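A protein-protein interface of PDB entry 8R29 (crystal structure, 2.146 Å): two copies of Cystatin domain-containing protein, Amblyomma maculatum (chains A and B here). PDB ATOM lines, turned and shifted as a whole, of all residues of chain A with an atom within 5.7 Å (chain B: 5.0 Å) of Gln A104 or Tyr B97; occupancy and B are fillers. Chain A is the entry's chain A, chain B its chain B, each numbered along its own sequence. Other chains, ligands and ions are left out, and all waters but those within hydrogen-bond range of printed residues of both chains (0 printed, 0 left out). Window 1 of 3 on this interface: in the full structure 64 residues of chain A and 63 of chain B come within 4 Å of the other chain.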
ATOM      1  N   VAL A  54     -25.403   9.796 -20.472  1.00  0.00           N
ATOM      2  CA  VAL A  54     -25.976   9.324 -21.729  1.00  0.00           C
ATOM      3  C   VAL A  54     -25.078   8.230 -22.262  1.00  0.00           C
ATOM      4  O   VAL A  54     -24.036   8.529 -22.797  1.00  0.00           O
ATOM      5  CB  VAL A  54     -26.188  10.397 -22.813  1.00  0.00           C
ATOM      6  CG1 VAL A  54     -26.944   9.823 -23.969  1.00  0.00           C
ATOM      7  CG2 VAL A  54     -26.951  11.594 -22.312  1.00  0.00           C
ATOM      8  N   ALA A  55     -25.538   6.985 -22.196  1.00  0.00           N
ATOM      9  CA  ALA A  55     -24.759   5.864 -22.671  1.00  0.00           C
ATOM     10  C   ALA A  55     -25.227   5.442 -24.067  1.00  0.00           C
ATOM     11  O   ALA A  55     -26.420   5.351 -24.375  1.00  0.00           O
ATOM     12  CB  ALA A  55     -24.870   4.707 -21.701  1.00  0.00           C
ATOM     13  N   GLY A  56     -24.226   5.130 -24.878  1.00  0.00           N
ATOM     14  CA  GLY A  56     -24.380   4.521 -26.190  1.00  0.00           C
ATOM     15  C   GLY A  56     -23.619   3.194 -26.284  1.00  0.00           C
ATOM     16  O   GLY A  56     -23.037   2.725 -25.283  1.00  0.00           O
ATOM     17  N   TYR A  97     -20.449   4.239 -33.514  1.00  0.00           N
ATOM     18  CA  TYR A  97     -21.007   4.610 -32.224  1.00  0.00           C
ATOM     19  C   TYR A  97     -22.484   4.978 -32.409  1.00  0.00           C
ATOM     20  O   TYR A  97     -22.834   5.884 -33.139  1.00  0.00           O
ATOM     21  CB  TYR A  97     -20.256   5.775 -31.614  1.00  0.00           C
ATOM     22  CG  TYR A  97     -20.628   6.149 -30.176  1.00  0.00           C
ATOM     23  CD1 TYR A  97     -20.653   5.205 -29.168  1.00  0.00           C
ATOM     24  CD2 TYR A  97     -20.828   7.473 -29.792  1.00  0.00           C
ATOM     25  CE1 TYR A  97     -21.013   5.517 -27.874  1.00  0.00           C
ATOM     26  CE2 TYR A  97     -21.081   7.821 -28.472  1.00  0.00           C
ATOM     27  CZ  TYR A  97     -21.218   6.837 -27.513  1.00  0.00           C
ATOM     28  OH  TYR A  97     -21.544   7.162 -26.203  1.00  0.00           O
ATOM     29  N   ASP A  98     -23.377   4.294 -31.707  1.00  0.00           N
ATOM     30  CA  ASP A  98     -24.811   4.501 -31.764  1.00  0.00           C
ATOM     31  C   ASP A  98     -25.291   5.048 -30.420  1.00  0.00           C
ATOM     32  O   ASP A  98     -25.032   4.433 -29.402  1.00  0.00           O
ATOM     33  CB  ASP A  98     -25.480   3.167 -32.095  1.00  0.00           C
ATOM     34  CG  ASP A  98     -26.913   3.291 -32.593  1.00  0.00           C
ATOM     35  OD1 ASP A  98     -27.208   4.192 -33.405  1.00  0.00           O
ATOM     36  OD2 ASP A  98     -27.721   2.514 -32.161  1.00  0.00           O
ATOM     37  N   VAL A  99     -25.941   6.217 -30.430  1.00  0.00           N
ATOM     38  CA  VAL A  99     -26.607   6.792 -29.266  1.00  0.00           C
ATOM     39  C   VAL A  99     -28.049   7.143 -29.640  1.00  0.00           C
ATOM     40  O   VAL A  99     -28.408   8.295 -29.909  1.00  0.00           O
ATOM     41  CB  VAL A  99     -25.879   8.039 -28.741  1.00  0.00           C
ATOM     42  CG1 VAL A  99     -26.356   8.403 -27.356  1.00  0.00           C
ATOM     43  CG2 VAL A  99     -24.353   7.880 -28.788  1.00  0.00           C
ATOM     44  N   PRO A 100     -28.960   6.159 -29.586  1.00  0.00           N
ATOM     45  CA  PRO A 100     -30.376   6.395 -29.830  1.00  0.00           C
ATOM     46  C   PRO A 100     -30.956   7.566 -29.065  1.00  0.00           C
ATOM     47  O   PRO A 100     -31.742   8.322 -29.633  1.00  0.00           O
ATOM     48  CB  PRO A 100     -31.038   5.106 -29.325  1.00  0.00           C
ATOM     49  CG  PRO A 100     -29.974   4.060 -29.446  1.00  0.00           C
ATOM     50  CD  PRO A 100     -28.704   4.800 -29.097  1.00  0.00           C
ATOM     51  N   LEU A 102     -30.016  10.370 -28.306  1.00  0.00           N
ATOM     52  CA  LEU A 102     -29.818  11.658 -28.964  1.00  0.00           C
ATOM     53  C   LEU A 102     -29.962  11.542 -30.489  1.00  0.00           C
ATOM     54  O   LEU A 102     -29.609  12.459 -31.220  1.00  0.00           O
ATOM     55  CB  LEU A 102     -28.404  12.131 -28.624  1.00  0.00           C
ATOM     56  CG  LEU A 102     -28.042  12.069 -27.162  1.00  0.00           C
ATOM     57  CD1 LEU A 102     -26.565  12.403 -27.005  1.00  0.00           C
ATOM     58  CD2 LEU A 102     -28.938  13.010 -26.348  1.00  0.00           C
ATOM     59  N   ASN A 103     -30.439  10.411 -30.969  1.00  0.00           N
ATOM     60  CA  ASN A 103     -30.498  10.122 -32.397  1.00  0.00           C
ATOM     61  C   ASN A 103     -29.202  10.548 -33.089  1.00  0.00           C
ATOM     62  O   ASN A 103     -29.179  11.313 -34.028  1.00  0.00           O
ATOM     63  CB  ASN A 103     -31.741  10.744 -33.020  1.00  0.00           C
ATOM     64  CG  ASN A 103     -32.194  10.018 -34.278  1.00  0.00           C
ATOM     65  OD1 ASN A 103     -32.276  10.637 -35.331  1.00  0.00           O
ATOM     66  ND2 ASN A 103     -32.516   8.733 -34.185  1.00  0.00           N
ATOM     67  N   GLN A 104     -28.102  10.121 -32.513  1.00  0.00           N
ATOM     68  CA  GLN A 104     -26.814  10.297 -33.122  1.00  0.00           C
ATOM     69  C   GLN A 104     -26.302   8.896 -33.429  1.00  0.00           C
ATOM     70  O   GLN A 104     -26.576   7.916 -32.747  1.00  0.00           O
ATOM     71  CB  GLN A 104     -25.901  11.034 -32.160  1.00  0.00           C
ATOM     72  CG  GLN A 104     -26.243  12.514 -31.997  1.00  0.00           C
ATOM     73  CD  GLN A 104     -25.291  13.150 -30.998  1.00  0.00           C
ATOM     74  OE1 GLN A 104     -24.308  12.545 -30.552  1.00  0.00           O
ATOM     75  NE2 GLN A 104     -25.585  14.374 -30.586  1.00  0.00           N
ATOM     76  N   ARG A 105     -25.573   8.814 -34.504  1.00  0.00           N
ATOM     77  CA  ARG A 105     -24.943   7.597 -34.938  1.00  0.00           C
ATOM     78  C   ARG A 105     -23.795   8.041 -35.839  1.00  0.00           C
ATOM     79  O   ARG A 105     -24.003   8.888 -36.681  1.00  0.00           O
ATOM     80  CB  ARG A 105     -25.983   6.769 -35.661  1.00  0.00           C
ATOM     81  CG  ARG A 105     -25.385   5.517 -36.260  1.00  0.00           C
ATOM     82  CD  ARG A 105     -26.454   4.789 -37.016  1.00  0.00           C
ATOM     83  NE  ARG A 105     -27.419   4.223 -36.104  1.00  0.00           N
ATOM     84  CZ  ARG A 105     -28.485   3.570 -36.530  1.00  0.00           C
ATOM     85  NH1 ARG A 105     -28.653   3.382 -37.829  1.00  0.00           N
ATOM     86  NH2 ARG A 105     -29.370   3.119 -35.666  1.00  0.00           N
ATOM     87  N   SER A 106     -22.588   7.536 -35.614  1.00  0.00           N
ATOM     88  CA  SER A 106     -21.440   7.984 -36.372  1.00  0.00           C
ATOM     89  C   SER A 106     -20.497   6.820 -36.653  1.00  0.00           C
ATOM     90  O   SER A 106     -20.407   5.907 -35.861  1.00  0.00           O
ATOM     91  CB  SER A 106     -20.786   9.079 -35.634  1.00  0.00           C
ATOM     92  OG  SER A 106     -20.481   8.635 -34.317  1.00  0.00           O
ATOM     93  N   VAL B  54     -20.370   2.734 -24.002  1.00  0.00           N
ATOM     94  CA  VAL B  54     -19.580   3.910 -23.728  1.00  0.00           C
ATOM     95  C   VAL B  54     -20.562   4.943 -23.228  1.00  0.00           C
ATOM     96  O   VAL B  54     -21.505   5.232 -23.950  1.00  0.00           O
ATOM     97  CB  VAL B  54     -18.846   4.438 -24.974  1.00  0.00           C
ATOM     98  CG1 VAL B  54     -17.914   5.612 -24.628  1.00  0.00           C
ATOM     99  CG2 VAL B  54     -18.048   3.360 -25.672  1.00  0.00           C
ATOM    100  N   ALA B  55     -20.355   5.434 -22.003  1.00  0.00           N
ATOM    101  CA  ALA B  55     -21.169   6.488 -21.460  1.00  0.00           C
ATOM    102  C   ALA B  55     -20.452   7.817 -21.594  1.00  0.00           C
ATOM    103  O   ALA B  55     -19.336   7.970 -21.127  1.00  0.00           O
ATOM    104  CB  ALA B  55     -21.462   6.219 -19.999  1.00  0.00           C
ATOM    105  N   GLY B  56     -21.133   8.778 -22.205  1.00  0.00           N
ATOM    106  CA  GLY B  56     -20.699  10.162 -22.229  1.00  0.00           C
ATOM    107  C   GLY B  56     -21.513  10.943 -21.207  1.00  0.00           C
ATOM    108  O   GLY B  56     -22.360  10.357 -20.567  1.00  0.00           O
ATOM    109  N   THR B  57     -21.264  12.256 -21.145  1.00  0.00           N
ATOM    110  CA  THR B  57     -21.972  13.147 -20.268  1.00  0.00           C
ATOM    111  C   THR B  57     -22.406  14.356 -21.060  1.00  0.00           C
ATOM    112  O   THR B  57     -21.602  14.956 -21.770  1.00  0.00           O
ATOM    113  CB  THR B  57     -21.130  13.591 -19.073  1.00  0.00           C
ATOM    114  OG1 THR B  57     -20.639  12.396 -18.480  1.00  0.00           O
ATOM    115  CG2 THR B  57     -21.915  14.366 -18.048  1.00  0.00           C
ATOM    116  N   ASN B  58     -23.688  14.687 -20.875  1.00  0.00           N
ATOM    117  CA  ASN B  58     -24.333  15.814 -21.502  1.00  0.00           C
ATOM    118  C   ASN B  58     -24.257  16.946 -20.493  1.00  0.00           C
ATOM    119  O   ASN B  58     -24.585  16.709 -19.335  1.00  0.00           O
ATOM    120  CB  ASN B  58     -25.765  15.420 -21.839  1.00  0.00           C
ATOM    121  CG  ASN B  58     -26.267  15.880 -23.198  1.00  0.00           C
ATOM    122  OD1 ASN B  58     -25.569  16.465 -24.028  1.00  0.00           O
ATOM    123  ND2 ASN B  58     -27.540  15.669 -23.411  1.00  0.00           N
ATOM    124  N   TYR B  59     -23.783  18.132 -20.909  1.00  0.00           N
ATOM    125  CA  TYR B  59     -23.592  19.237 -19.984  1.00  0.00           C
ATOM    126  C   TYR B  59     -24.485  20.386 -20.425  1.00  0.00           C
ATOM    127  O   TYR B  59     -24.414  20.763 -21.591  1.00  0.00           O
ATOM    128  CB  TYR B  59     -22.143  19.721 -19.896  1.00  0.00           C
ATOM    129  CG  TYR B  59     -21.116  18.702 -19.425  1.00  0.00           C
ATOM    130  CD1 TYR B  59     -20.611  17.739 -20.271  1.00  0.00           C
ATOM    131  CD2 TYR B  59     -20.706  18.658 -18.105  1.00  0.00           C
ATOM    132  CE1 TYR B  59     -19.703  16.789 -19.838  1.00  0.00           C
ATOM    133  CE2 TYR B  59     -19.828  17.688 -17.645  1.00  0.00           C
ATOM    134  CZ  TYR B  59     -19.312  16.754 -18.516  1.00  0.00           C
ATOM    135  OH  TYR B  59     -18.426  15.818 -18.046  1.00  0.00           O
ATOM    136  N   VAL B  95     -25.823  23.254 -24.488  1.00  0.00           N
ATOM    137  CA  VAL B  95     -25.747  21.850 -24.112  1.00  0.00           C
ATOM    138  C   VAL B  95     -24.605  21.202 -24.877  1.00  0.00           C
ATOM    139  O   VAL B  95     -24.597  21.301 -26.104  1.00  0.00           O
ATOM    140  CB  VAL B  95     -27.065  21.133 -24.447  1.00  0.00           C
ATOM    141  CG1 VAL B  95     -27.008  19.672 -24.019  1.00  0.00           C
ATOM    142  CG2 VAL B  95     -28.285  21.858 -23.871  1.00  0.00           C
ATOM    143  N   ILE B  96     -23.658  20.594 -24.156  1.00  0.00           N
ATOM    144  CA  ILE B  96     -22.519  19.925 -24.783  1.00  0.00           C
ATOM    145  C   ILE B  96     -22.479  18.462 -24.415  1.00  0.00           C
ATOM    146  O   ILE B  96     -22.361  18.180 -23.233  1.00  0.00           O
ATOM    147  CB  ILE B  96     -21.174  20.530 -24.338  1.00  0.00           C
ATOM    148  CG1 ILE B  96     -21.027  22.020 -24.673  1.00  0.00           C
ATOM    149  CG2 ILE B  96     -20.036  19.723 -24.895  1.00  0.00           C
ATOM    150  CD1 ILE B  96     -21.111  22.911 -23.454  1.00  0.00           C
ATOM    151  N   TYR B  97     -22.469  17.574 -25.414  1.00  0.00           N
ATOM    152  CA  TYR B  97     -22.242  16.155 -25.186  1.00  0.00           C
ATOM    153  C   TYR B  97     -20.752  15.846 -25.328  1.00  0.00           C
ATOM    154  O   TYR B  97     -20.215  15.999 -26.399  1.00  0.00           O
ATOM    155  CB  TYR B  97     -23.086  15.311 -26.145  1.00  0.00           C
ATOM    156  CG  TYR B  97     -23.025  13.799 -25.943  1.00  0.00           C
ATOM    157  CD1 TYR B  97     -23.233  13.237 -24.686  1.00  0.00           C
ATOM    158  CD2 TYR B  97     -22.807  12.913 -27.018  1.00  0.00           C
ATOM    159  CE1 TYR B  97     -23.189  11.861 -24.506  1.00  0.00           C
ATOM    160  CE2 TYR B  97     -22.783  11.529 -26.842  1.00  0.00           C
ATOM    161  CZ  TYR B  97     -22.982  10.992 -25.578  1.00  0.00           C
ATOM    162  OH  TYR B  97     -22.969   9.616 -25.306  1.00  0.00           O
ATOM    163  N   ASP B  98     -20.141  15.325 -24.256  1.00  0.00           N
ATOM    164  CA  ASP B  98     -18.727  15.026 -24.181  1.00  0.00           C
ATOM    165  C   ASP B  98     -18.543  13.517 -24.028  1.00  0.00           C
ATOM    166  O   ASP B  98     -19.132  12.915 -23.131  1.00  0.00           O
ATOM    167  CB  ASP B  98     -18.108  15.776 -23.006  1.00  0.00           C
ATOM    168  CG  ASP B  98     -16.589  15.857 -23.059  1.00  0.00           C
ATOM    169  OD1 ASP B  98     -16.040  16.190 -24.130  1.00  0.00           O
ATOM    170  OD2 ASP B  98     -15.975  15.600 -22.024  1.00  0.00           O
ATOM    171  N   VAL B  99     -17.796  12.919 -24.981  1.00  0.00           N
ATOM    172  CA  VAL B  99     -17.369  11.532 -24.902  1.00  0.00           C
ATOM    173  C   VAL B  99     -15.847  11.455 -25.019  1.00  0.00           C
ATOM    174  O   VAL B  99     -15.345  11.179 -26.076  1.00  0.00           O
ATOM    175  CB  VAL B  99     -18.049  10.682 -25.974  1.00  0.00           C
ATOM    176  CG1 VAL B  99     -18.004   9.240 -25.506  1.00  0.00           C
ATOM    177  CG2 VAL B  99     -19.481  11.120 -26.252  1.00  0.00           C
ATOM    178  N   GLN B 104     -14.842  12.700 -28.841  1.00  0.00           N
ATOM    179  CA  GLN B 104     -15.916  13.370 -29.522  1.00  0.00           C
ATOM    180  C   GLN B 104     -16.471  14.401 -28.554  1.00  0.00           C
ATOM    181  O   GLN B 104     -16.459  14.184 -27.353  1.00  0.00           O
ATOM    182  CB  GLN B 104     -16.921  12.314 -29.963  1.00  0.00           C
ATOM    183  CG  GLN B 104     -16.354  11.503 -31.093  1.00  0.00           C
ATOM    184  CD  GLN B 104     -17.241  10.397 -31.573  1.00  0.00           C
ATOM    185  OE1 GLN B 104     -18.455  10.404 -31.354  1.00  0.00           O
ATOM    186  NE2 GLN B 104     -16.597   9.446 -32.256  1.00  0.00           N
ATOM    187  N   ARG B 105     -16.833  15.542 -29.115  1.00  0.00           N
ATOM    188  CA  ARG B 105     -17.455  16.568 -28.336  1.00  0.00           C
ATOM    189  C   ARG B 105     -18.333  17.365 -29.270  1.00  0.00           C
ATOM    190  O   ARG B 105     -17.892  17.666 -30.354  1.00  0.00           O
ATOM    191  CB  ARG B 105     -16.386  17.445 -27.712  1.00  0.00           C
ATOM    192  CG  ARG B 105     -17.041  18.498 -26.858  1.00  0.00           C
ATOM    193  CD  ARG B 105     -16.014  19.298 -26.117  1.00  0.00           C
ATOM    194  NE  ARG B 105     -15.243  18.521 -25.190  1.00  0.00           N
ATOM    195  CZ  ARG B 105     -14.138  18.986 -24.611  1.00  0.00           C
ATOM    196  NH1 ARG B 105     -13.678  20.180 -24.936  1.00  0.00           N
ATOM    197  NH2 ARG B 105     -13.543  18.294 -23.659  1.00  0.00           N
ATOM    198  N   SER B 106     -19.557  17.688 -28.847  1.00  0.00           N
ATOM    199  CA  SER B 106     -20.500  18.334 -29.735  1.00  0.00           C
ATOM    200  C   SER B 106     -21.380  19.267 -28.933  1.00  0.00           C
ATOM    201  O   SER B 106     -21.629  19.039 -27.763  1.00  0.00           O
ATOM    202  CB  SER B 106     -21.309  17.348 -30.490  1.00  0.00           C
ATOM    203  OG  SER B 106     -22.421  16.879 -29.735  1.00  0.00           O
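The backbone carbonyl oxygen (O) of Val A54 is in hydrogen-bond range of the backbone NH (N) of Gly B56 (3.0 Å). O of Val A54 is in hydrogen-bond range of OH of Tyr B97 (2.9 Å). O of Val B54 sits at hydrogen-bond distance from N of Gly A56. The backbone carbonyl oxygen of Val B54 sits at hydrogen-bond distance from the side-chain hydroxyl of Tyr A97 (3.0 Å). OH of Tyr A97 is in hydrogen-bond range of OH of Tyr B97, 3.0 Å away.
The backbone NH (N) of Tyr A97 lies within hydrogen-bond range of the backbone carbonyl oxygen (O) of Ser A106, at 2.9 Å. The backbone NH (N) of Val A99 sits at hydrogen-bond distance from the backbone carbonyl oxygen (O) of Gln A104 (2.9 Å). O of Ser B106 is in hydrogen-bond range of N of Tyr B97 (2.9 Å).
Among the printed residues, pairs that only touch across the chains: Ala A55 with Val B54, Val A54 with Ala B55, Leu A102 with Tyr B97, Ala A55 with Ala B55 and Gln A104 with Tyr B97.
Of the printed residues of chain B, Ala A55 touches Val B54 and Ala B55. Asp A98 touches none of the printed residues of chain B. Of the printed residues of chain B, Leu A102 touches Tyr B97 (3.8 Å). Gln A104 touches just one residue of chain B: Tyr B97 (3.9 Å). Printed residues of chain A within 4 Å of Gly B56: Val A54 (3.0 Å). Of chain A, only Val A54, Tyr A97, Leu A102 and Gln A104 come within 4 Å of Tyr B97. Asp B98 touches none of the printed residues of chain A.
Of the 12 printed residues of chain A, 6 touch a printed residue of chain B. Hydrophobic or aromatic side chains of chain A within 4 Å of the printed part of chain B: Val A54, Tyr A97 and Leu A102. Of the 14 printed residues of chain B, 4 touch a printed residue of chain A. Among the printed residues, 10 pairs touch across the chains. Among the printed residues, no Asp or Glu carboxylate lies within 4 Å of a Lys or Arg side-chain nitrogen of the other chain.
Val A54 touches Ala B55, and with the chains exchanged Ala A55 touches Val B54. Val A54 touches Gly B56, and with the chains exchanged Gly A56 touches Val B54. Tyr B97 touches its own counterpart, Tyr A97. Gln A104 touches Tyr B97, but with the chains exchanged Tyr A97 does not touch Gln B104 (4.1 Å).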
